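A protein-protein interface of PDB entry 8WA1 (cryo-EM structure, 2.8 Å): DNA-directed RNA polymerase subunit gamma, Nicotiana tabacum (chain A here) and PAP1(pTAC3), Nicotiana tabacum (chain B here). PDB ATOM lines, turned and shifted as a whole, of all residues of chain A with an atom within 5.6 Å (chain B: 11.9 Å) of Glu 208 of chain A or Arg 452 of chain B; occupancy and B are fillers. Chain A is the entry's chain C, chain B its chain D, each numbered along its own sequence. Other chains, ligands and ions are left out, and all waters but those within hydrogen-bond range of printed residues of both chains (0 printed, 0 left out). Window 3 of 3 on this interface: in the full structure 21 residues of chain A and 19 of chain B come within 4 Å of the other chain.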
ATOM      1  N   PRO A 157      12.597 -13.597  -5.289  1.00  0.00           N
ATOM      2  CA  PRO A 157      14.034 -13.881  -5.245  1.00  0.00           C
ATOM      3  C   PRO A 157      14.588 -14.098  -3.847  1.00  0.00           C
ATOM      4  O   PRO A 157      15.717 -14.594  -3.721  1.00  0.00           O
ATOM      5  CB  PRO A 157      14.645 -12.623  -5.881  1.00  0.00           C
ATOM      6  N   ILE A 158      13.839 -13.745  -2.806  1.00  0.00           N
ATOM      7  CA  ILE A 158      14.274 -13.896  -1.423  1.00  0.00           C
ATOM      8  C   ILE A 158      13.313 -14.845  -0.722  1.00  0.00           C
ATOM      9  O   ILE A 158      12.091 -14.693  -0.833  1.00  0.00           O
ATOM     10  CB  ILE A 158      14.331 -12.541  -0.693  1.00  0.00           C
ATOM     11  CG1 ILE A 158      15.195 -11.551  -1.476  1.00  0.00           C
ATOM     12  CG2 ILE A 158      14.871 -12.720   0.716  1.00  0.00           C
ATOM     13  CD1 ILE A 158      15.248 -10.170  -0.861  1.00  0.00           C
ATOM     14  N   LYS A 160      14.079 -15.748   2.712  1.00  0.00           N
ATOM     15  CA  LYS A 160      14.366 -15.598   4.134  1.00  0.00           C
ATOM     16  C   LYS A 160      13.799 -14.306   4.709  1.00  0.00           C
ATOM     17  O   LYS A 160      14.162 -13.926   5.828  1.00  0.00           O
ATOM     18  CB  LYS A 160      15.876 -15.667   4.382  1.00  0.00           C
ATOM     19  CG  LYS A 160      16.508 -16.989   3.974  1.00  0.00           C
ATOM     20  CD  LYS A 160      17.990 -17.027   4.309  1.00  0.00           C
ATOM     21  CE  LYS A 160      18.612 -18.358   3.914  1.00  0.00           C
ATOM     22  NZ  LYS A 160      20.057 -18.428   4.263  1.00  0.00           N
ATOM     23  N   ASN A 196      12.790  -5.304  -3.651  1.00  0.00           N
ATOM     24  CA  ASN A 196      13.810  -6.346  -3.695  1.00  0.00           C
ATOM     25  C   ASN A 196      13.268  -7.685  -3.215  1.00  0.00           C
ATOM     26  O   ASN A 196      13.554  -8.719  -3.829  1.00  0.00           O
ATOM     27  CB  ASN A 196      15.019  -5.936  -2.853  1.00  0.00           C
ATOM     28  N   GLY A 204      19.617  -8.936  -9.750  1.00  0.00           N
ATOM     29  CA  GLY A 204      19.396  -9.027  -8.319  1.00  0.00           C
ATOM     30  C   GLY A 204      18.755 -10.327  -7.883  1.00  0.00           C
ATOM     31  O   GLY A 204      19.049 -10.817  -6.786  1.00  0.00           O
ATOM     32  N   ALA A 205      17.898 -10.903  -8.727  1.00  0.00           N
ATOM     33  CA  ALA A 205      17.247 -12.162  -8.387  1.00  0.00           C
ATOM     34  C   ALA A 205      18.261 -13.289  -8.258  1.00  0.00           C
ATOM     35  O   ALA A 205      18.179 -14.105  -7.333  1.00  0.00           O
ATOM     36  CB  ALA A 205      16.191 -12.505  -9.436  1.00  0.00           C
ATOM     37  N   ILE A 206      19.224 -13.354  -9.180  1.00  0.00           N
ATOM     38  CA  ILE A 206      20.230 -14.409  -9.127  1.00  0.00           C
ATOM     39  C   ILE A 206      21.066 -14.288  -7.860  1.00  0.00           C
ATOM     40  O   ILE A 206      21.335 -15.286  -7.179  1.00  0.00           O
ATOM     41  CB  ILE A 206      21.110 -14.372 -10.390  1.00  0.00           C
ATOM     42  CG1 ILE A 206      20.243 -14.485 -11.644  1.00  0.00           C
ATOM     43  CG2 ILE A 206      22.146 -15.485 -10.351  1.00  0.00           C
ATOM     44  CD1 ILE A 206      19.392 -15.733 -11.683  1.00  0.00           C
ATOM     45  N   ARG A 207      21.482 -13.067  -7.518  1.00  0.00           N
ATOM     46  CA  ARG A 207      22.299 -12.876  -6.325  1.00  0.00           C
ATOM     47  C   ARG A 207      21.516 -13.199  -5.060  1.00  0.00           C
ATOM     48  O   ARG A 207      22.059 -13.792  -4.120  1.00  0.00           O
ATOM     49  CB  ARG A 207      22.839 -11.446  -6.278  1.00  0.00           C
ATOM     50  CG  ARG A 207      23.469 -11.062  -4.948  1.00  0.00           C
ATOM     51  CD  ARG A 207      24.342  -9.823  -5.072  1.00  0.00           C
ATOM     52  NE  ARG A 207      25.631 -10.124  -5.688  1.00  0.00           N
ATOM     53  CZ  ARG A 207      26.704 -10.529  -5.015  1.00  0.00           C
ATOM     54  NH1 ARG A 207      26.642 -10.683  -3.699  1.00  0.00           N
ATOM     55  NH2 ARG A 207      27.838 -10.780  -5.655  1.00  0.00           N
ATOM     56  N   GLU A 208      20.233 -12.830  -5.016  1.00  0.00           N
ATOM     57  CA  GLU A 208      19.435 -13.132  -3.830  1.00  0.00           C
ATOM     58  C   GLU A 208      19.161 -14.627  -3.708  1.00  0.00           C
ATOM     59  O   GLU A 208      19.110 -15.164  -2.596  1.00  0.00           O
ATOM     60  CB  GLU A 208      18.132 -12.335  -3.849  1.00  0.00           C
ATOM     61  CG  GLU A 208      18.305 -10.826  -3.665  1.00  0.00           C
ATOM     62  CD  GLU A 208      19.133 -10.456  -2.442  1.00  0.00           C
ATOM     63  OE1 GLU A 208      20.380 -10.497  -2.524  1.00  0.00           O
ATOM     64  OE2 GLU A 208      18.538 -10.119  -1.396  1.00  0.00           O
ATOM     65  N   GLN A 209      18.983 -15.320  -4.836  1.00  0.00           N
ATOM     66  CA  GLN A 209      18.782 -16.765  -4.791  1.00  0.00           C
ATOM     67  C   GLN A 209      20.049 -17.479  -4.335  1.00  0.00           C
ATOM     68  O   GLN A 209      19.991 -18.404  -3.515  1.00  0.00           O
ATOM     69  CB  GLN A 209      18.333 -17.283  -6.158  1.00  0.00           C
ATOM     70  CG  GLN A 209      16.900 -16.930  -6.533  1.00  0.00           C
ATOM     71  CD  GLN A 209      15.870 -17.664  -5.694  1.00  0.00           C
ATOM     72  OE1 GLN A 209      16.184 -18.644  -5.017  1.00  0.00           O
ATOM     73  NE2 GLN A 209      14.630 -17.192  -5.737  1.00  0.00           N
ATOM     74  N   LEU A 210      21.205 -17.064  -4.858  1.00  0.00           N
ATOM     75  CA  LEU A 210      22.462 -17.686  -4.449  1.00  0.00           C
ATOM     76  C   LEU A 210      22.788 -17.373  -2.993  1.00  0.00           C
ATOM     77  O   LEU A 210      23.364 -18.208  -2.287  1.00  0.00           O
ATOM     78  CB  LEU A 210      23.595 -17.231  -5.370  1.00  0.00           C
ATOM     79  CG  LEU A 210      23.447 -17.633  -6.840  1.00  0.00           C
ATOM     80  CD1 LEU A 210      24.571 -17.049  -7.682  1.00  0.00           C
ATOM     81  CD2 LEU A 210      23.395 -19.145  -6.977  1.00  0.00           C
ATOM     82  N   ALA A 211      22.434 -16.171  -2.529  1.00  0.00           N
ATOM     83  CA  ALA A 211      22.743 -15.787  -1.157  1.00  0.00           C
ATOM     84  C   ALA A 211      21.789 -16.446  -0.168  1.00  0.00           C
ATOM     85  O   ALA A 211      22.225 -17.115   0.778  1.00  0.00           O
ATOM     86  CB  ALA A 211      22.694 -14.266  -1.016  1.00  0.00           C
ATOM     87  N   ASP A 212      20.486 -16.273  -0.371  1.00  0.00           N
ATOM     88  CA  ASP A 212      19.468 -16.821   0.520  1.00  0.00           C
ATOM     89  C   ASP A 212      19.173 -18.244   0.062  1.00  0.00           C
ATOM     90  O   ASP A 212      18.238 -18.481  -0.708  1.00  0.00           O
ATOM     91  CB  ASP A 212      18.216 -15.952   0.511  1.00  0.00           C
ATOM     92  CG  ASP A 212      18.502 -14.512   0.889  1.00  0.00           C
ATOM     93  OD1 ASP A 212      19.212 -13.825   0.123  1.00  0.00           O
ATOM     94  OD2 ASP A 212      18.017 -14.065   1.949  1.00  0.00           O
ATOM     95  N   LEU A 213      19.973 -19.191   0.543  1.00  0.00           N
ATOM     96  CA  LEU A 213      19.834 -20.583   0.144  1.00  0.00           C
ATOM     97  C   LEU A 213      20.464 -21.460   1.213  1.00  0.00           C
ATOM     98  O   LEU A 213      21.510 -21.130   1.779  1.00  0.00           O
ATOM     99  CB  LEU A 213      20.481 -20.837  -1.222  1.00  0.00           C
ATOM    100  CG  LEU A 213      20.120 -22.143  -1.929  1.00  0.00           C
ATOM    101  CD1 LEU A 213      18.637 -22.169  -2.259  1.00  0.00           C
ATOM    102  CD2 LEU A 213      20.956 -22.318  -3.186  1.00  0.00           C
ATOM    103  N   GLU A 269      27.575 -16.981  -3.644  1.00  0.00           N
ATOM    104  CA  GLU A 269      27.299 -15.572  -3.902  1.00  0.00           C
ATOM    105  C   GLU A 269      28.356 -14.955  -4.808  1.00  0.00           C
ATOM    106  O   GLU A 269      28.073 -14.011  -5.555  1.00  0.00           O
ATOM    107  CB  GLU A 269      27.227 -14.806  -2.582  1.00  0.00           C
ATOM    108  CG  GLU A 269      26.213 -15.357  -1.601  1.00  0.00           C
ATOM    109  CD  GLU A 269      26.329 -14.728  -0.227  1.00  0.00           C
ATOM    110  OE1 GLU A 269      27.112 -15.237   0.600  1.00  0.00           O
ATOM    111  OE2 GLU A 269      25.641 -13.717   0.024  1.00  0.00           O
ATOM    112  N   ARG B 447      17.065 -17.782  19.159  1.00  0.00           N
ATOM    113  CA  ARG B 447      16.027 -17.258  18.310  1.00  0.00           C
ATOM    114  C   ARG B 447      16.065 -17.977  16.984  1.00  0.00           C
ATOM    115  O   ARG B 447      17.057 -17.903  16.272  1.00  0.00           O
ATOM    116  CB  ARG B 447      16.237 -15.770  18.109  1.00  0.00           C
ATOM    117  CG  ARG B 447      15.991 -14.942  19.353  1.00  0.00           C
ATOM    118  CD  ARG B 447      17.253 -14.233  19.810  1.00  0.00           C
ATOM    119  NE  ARG B 447      16.985 -13.324  20.920  1.00  0.00           N
ATOM    120  CZ  ARG B 447      16.665 -12.044  20.776  1.00  0.00           C
ATOM    121  NH1 ARG B 447      16.576 -11.509  19.566  1.00  0.00           N
ATOM    122  NH2 ARG B 447      16.437 -11.294  21.844  1.00  0.00           N
ATOM    123  N   TRP B 448      14.995 -18.674  16.643  1.00  0.00           N
ATOM    124  CA  TRP B 448      14.984 -19.446  15.418  1.00  0.00           C
ATOM    125  C   TRP B 448      14.718 -18.593  14.197  1.00  0.00           C
ATOM    126  O   TRP B 448      13.602 -18.570  13.686  1.00  0.00           O
ATOM    127  CB  TRP B 448      13.960 -20.570  15.527  1.00  0.00           C
ATOM    128  CG  TRP B 448      14.272 -21.544  16.627  1.00  0.00           C
ATOM    129  CD1 TRP B 448      14.187 -21.323  17.971  1.00  0.00           C
ATOM    130  CD2 TRP B 448      14.718 -22.894  16.472  1.00  0.00           C
ATOM    131  NE1 TRP B 448      14.558 -22.447  18.661  1.00  0.00           N
ATOM    132  CE2 TRP B 448      14.885 -23.428  17.765  1.00  0.00           C
ATOM    133  CE3 TRP B 448      14.991 -23.703  15.369  1.00  0.00           C
ATOM    134  CZ2 TRP B 448      15.315 -24.732  17.981  1.00  0.00           C
ATOM    135  CZ3 TRP B 448      15.416 -24.997  15.585  1.00  0.00           C
ATOM    136  CH2 TRP B 448      15.572 -25.499  16.880  1.00  0.00           C
ATOM    137  N   VAL B 449      15.749 -17.905  13.716  1.00  0.00           N
ATOM    138  CA  VAL B 449      15.599 -17.080  12.520  1.00  0.00           C
ATOM    139  C   VAL B 449      16.656 -17.497  11.504  1.00  0.00           C
ATOM    140  O   VAL B 449      17.845 -17.590  11.845  1.00  0.00           O
ATOM    141  CB  VAL B 449      15.691 -15.582  12.856  1.00  0.00           C
ATOM    142  CG1 VAL B 449      16.908 -15.294  13.727  1.00  0.00           C
ATOM    143  CG2 VAL B 449      15.730 -14.751  11.581  1.00  0.00           C
ATOM    144  N   PRO B 450      16.272 -17.782  10.260  1.00  0.00           N
ATOM    145  CA  PRO B 450      17.265 -18.183   9.253  1.00  0.00           C
ATOM    146  C   PRO B 450      18.189 -17.024   8.905  1.00  0.00           C
ATOM    147  O   PRO B 450      17.752 -15.877   8.782  1.00  0.00           O
ATOM    148  CB  PRO B 450      16.407 -18.601   8.053  1.00  0.00           C
ATOM    149  CG  PRO B 450      15.040 -18.853   8.619  1.00  0.00           C
ATOM    150  CD  PRO B 450      14.896 -17.887   9.752  1.00  0.00           C
ATOM    151  N   ARG B 451      19.473 -17.333   8.746  1.00  0.00           N
ATOM    152  CA  ARG B 451      20.481 -16.344   8.399  1.00  0.00           C
ATOM    153  C   ARG B 451      21.110 -16.700   7.060  1.00  0.00           C
ATOM    154  O   ARG B 451      21.045 -17.844   6.602  1.00  0.00           O
ATOM    155  CB  ARG B 451      21.565 -16.236   9.482  1.00  0.00           C
ATOM    156  CG  ARG B 451      21.071 -15.635  10.789  1.00  0.00           C
ATOM    157  CD  ARG B 451      20.473 -14.253  10.565  1.00  0.00           C
ATOM    158  NE  ARG B 451      19.946 -13.670  11.795  1.00  0.00           N
ATOM    159  CZ  ARG B 451      19.326 -12.497  11.860  1.00  0.00           C
ATOM    160  NH1 ARG B 451      19.151 -11.776  10.761  1.00  0.00           N
ATOM    161  NH2 ARG B 451      18.878 -12.043  13.023  1.00  0.00           N
ATOM    162  N   ARG B 452      21.724 -15.695   6.433  1.00  0.00           N
ATOM    163  CA  ARG B 452      22.302 -15.891   5.107  1.00  0.00           C
ATOM    164  C   ARG B 452      23.572 -16.731   5.170  1.00  0.00           C
ATOM    165  O   ARG B 452      23.847 -17.520   4.257  1.00  0.00           O
ATOM    166  CB  ARG B 452      22.581 -14.534   4.459  1.00  0.00           C
ATOM    167  CG  ARG B 452      23.233 -14.610   3.089  1.00  0.00           C
ATOM    168  CD  ARG B 452      23.222 -13.253   2.409  1.00  0.00           C
ATOM    169  NE  ARG B 452      21.862 -12.781   2.169  1.00  0.00           N
ATOM    170  CZ  ARG B 452      21.563 -11.648   1.542  1.00  0.00           C
ATOM    171  NH1 ARG B 452      22.531 -10.864   1.088  1.00  0.00           N
ATOM    172  NH2 ARG B 452      20.296 -11.298   1.369  1.00  0.00           N
ATOM    173  N   GLY B 453      24.354 -16.582   6.235  1.00  0.00           N
ATOM    174  CA  GLY B 453      25.611 -17.293   6.347  1.00  0.00           C
ATOM    175  C   GLY B 453      25.434 -18.798   6.425  1.00  0.00           C
ATOM    176  O   GLY B 453      24.373 -19.325   6.762  1.00  0.00           O
ATOM    177  N   LYS B 454      26.517 -19.504   6.100  1.00  0.00           N
ATOM    178  CA  LYS B 454      26.520 -20.968   6.098  1.00  0.00           C
ATOM    179  C   LYS B 454      26.752 -21.476   7.521  1.00  0.00           C
ATOM    180  O   LYS B 454      27.796 -22.035   7.866  1.00  0.00           O
ATOM    181  CB  LYS B 454      27.570 -21.500   5.132  1.00  0.00           C
ATOM    182  CG  LYS B 454      27.333 -21.116   3.681  1.00  0.00           C
ATOM    183  CD  LYS B 454      28.362 -21.757   2.764  1.00  0.00           C
ATOM    184  CE  LYS B 454      29.777 -21.371   3.163  1.00  0.00           C
ATOM    185  NZ  LYS B 454      30.793 -22.020   2.291  1.00  0.00           N
ATOM    186  N   THR B 455      25.737 -21.272   8.358  1.00  0.00           N
ATOM    187  CA  THR B 455      25.755 -21.700   9.745  1.00  0.00           C
ATOM    188  C   THR B 455      24.395 -22.292  10.084  1.00  0.00           C
ATOM    189  O   THR B 455      23.363 -21.642   9.862  1.00  0.00           O
ATOM    190  CB  THR B 455      26.067 -20.540  10.702  1.00  0.00           C
ATOM    191  OG1 THR B 455      27.347 -19.982  10.382  1.00  0.00           O
ATOM    192  CG2 THR B 455      26.075 -21.023  12.143  1.00  0.00           C
ATOM    193  N   PRO B 456      24.358 -23.513  10.614  1.00  0.00           N
ATOM    194  CA  PRO B 456      23.066 -24.135  10.925  1.00  0.00           C
ATOM    195  C   PRO B 456      22.389 -23.456  12.106  1.00  0.00           C
ATOM    196  O   PRO B 456      22.968 -23.321  13.186  1.00  0.00           O
ATOM    197  CB  PRO B 456      23.441 -25.585  11.250  1.00  0.00           C
ATOM    198  CG  PRO B 456      24.859 -25.511  11.709  1.00  0.00           C
ATOM    199  CD  PRO B 456      25.492 -24.405  10.912  1.00  0.00           C
ATOM    200  N   LEU B 457      21.145 -23.025  11.886  1.00  0.00           N
ATOM    201  CA  LEU B 457      20.383 -22.402  12.963  1.00  0.00           C
ATOM    202  C   LEU B 457      19.970 -23.433  14.005  1.00  0.00           C
ATOM    203  O   LEU B 457      19.825 -23.105  15.188  1.00  0.00           O
ATOM    204  CB  LEU B 457      19.163 -21.658  12.400  1.00  0.00           C
ATOM    205  CG  LEU B 457      18.007 -22.281  11.590  1.00  0.00           C
ATOM    206  CD1 LEU B 457      18.469 -23.032  10.338  1.00  0.00           C
ATOM    207  CD2 LEU B 457      17.077 -23.151  12.440  1.00  0.00           C
ATOM    208  N   ASP B 458      19.777 -24.678  13.588  1.00  0.00           N
ATOM    209  CA  ASP B 458      19.466 -25.734  14.535  1.00  0.00           C
ATOM    210  C   ASP B 458      20.724 -26.125  15.306  1.00  0.00           C
ATOM    211  O   ASP B 458      21.780 -26.342  14.704  1.00  0.00           O
ATOM    212  CB  ASP B 458      18.890 -26.950  13.810  1.00  0.00           C
ATOM    213  CG  ASP B 458      18.542 -28.082  14.752  1.00  0.00           C
ATOM    214  OD1 ASP B 458      17.609 -27.916  15.565  1.00  0.00           O
ATOM    215  OD2 ASP B 458      19.197 -29.139  14.674  1.00  0.00           O
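Among the printed residues, merely in contact across the chains: Lys 160 of chain A with Arg 452 of chain B, Ala 211 of chain A with Arg 452 of chain B and Glu 269 of chain A with Arg 452 of chain B.
NZ of Lys 160 of chain A lies within hydrogen-bond range of O of Arg 451 of chain B (2.6 Å). OE2 of Glu 208 of chain A lies within salt-bridge range of NH2 of Arg 452 of chain B, 3.5 Å away. The guanidinium group (NH2) of Arg 452 of chain B lies within salt-bridge range of the side-chain carboxylate (OD1) of Asp 212 of chain A.
The guanidinium group (NH2) of Arg 207 of chain A lies within hydrogen-bond range of the backbone carbonyl oxygen (O) of Glu 269 of chain A.
Hydrophobic or aromatic side chains of chain A within 4 Å of the printed part of chain B: Ala 211. Of the 12 printed residues of chain B, 2 touch a printed residue of chain A. Among the printed residues, Asp or Glu carboxylates within 4 Å of a Lys or Arg side-chain nitrogen of the other chain: Glu 208 of chain A with Arg 452 of chain B (3.5 Å) and Asp 212 of chain A with Arg 452 of chain B (3.0 Å).
Of chain B, only Arg 452 comes within 4 Å of Glu 208 of chain A. No residue of chain B comes within 4 Å of Pro 157 of chain A. No residue of chain B comes within 4 Å of Ile 158 of chain A. No residue of chain B comes within 4 Å of Asn 196 of chain A. No residue of chain B comes within 4 Å of Gly 204 of chain A. No residue of chain B comes within 4 Å of Ala 205 of chain A. No residue of chain B comes within 4 Å of Ile 206 of chain A. No residue of chain B comes within 4 Å of Gln 209 of chain A. No residue of chain B comes within 4 Å of Leu 210 of chain A. Ala 211 of chain A touches one residue of chain B. Asp 212 of chain A touches just one residue of chain B: Arg 452. No residue of chain B comes within 4 Å of Leu 213 of chain A. Printed residues of chain B within 4 Å of Lys 160 of chain A: Arg 451 and Arg 452. Of the printed residues of chain B, Glu 269 of chain A touches Arg 452. Printed residues of chain A within 4 Å of Arg 451 of chain B: Lys 160. Leu 457 of chain B touches none of the printed residues of chain A. Lys 454 of chain B touches none of the printed residues of chain A. The nearest residue of chain B that does not touch Glu 208 of chain A is Arg 451 of chain B (9.8 Å). The nearest residue of chain A that does not touch Arg 452 of chain B is Leu 213 of chain A (5.0 Å).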
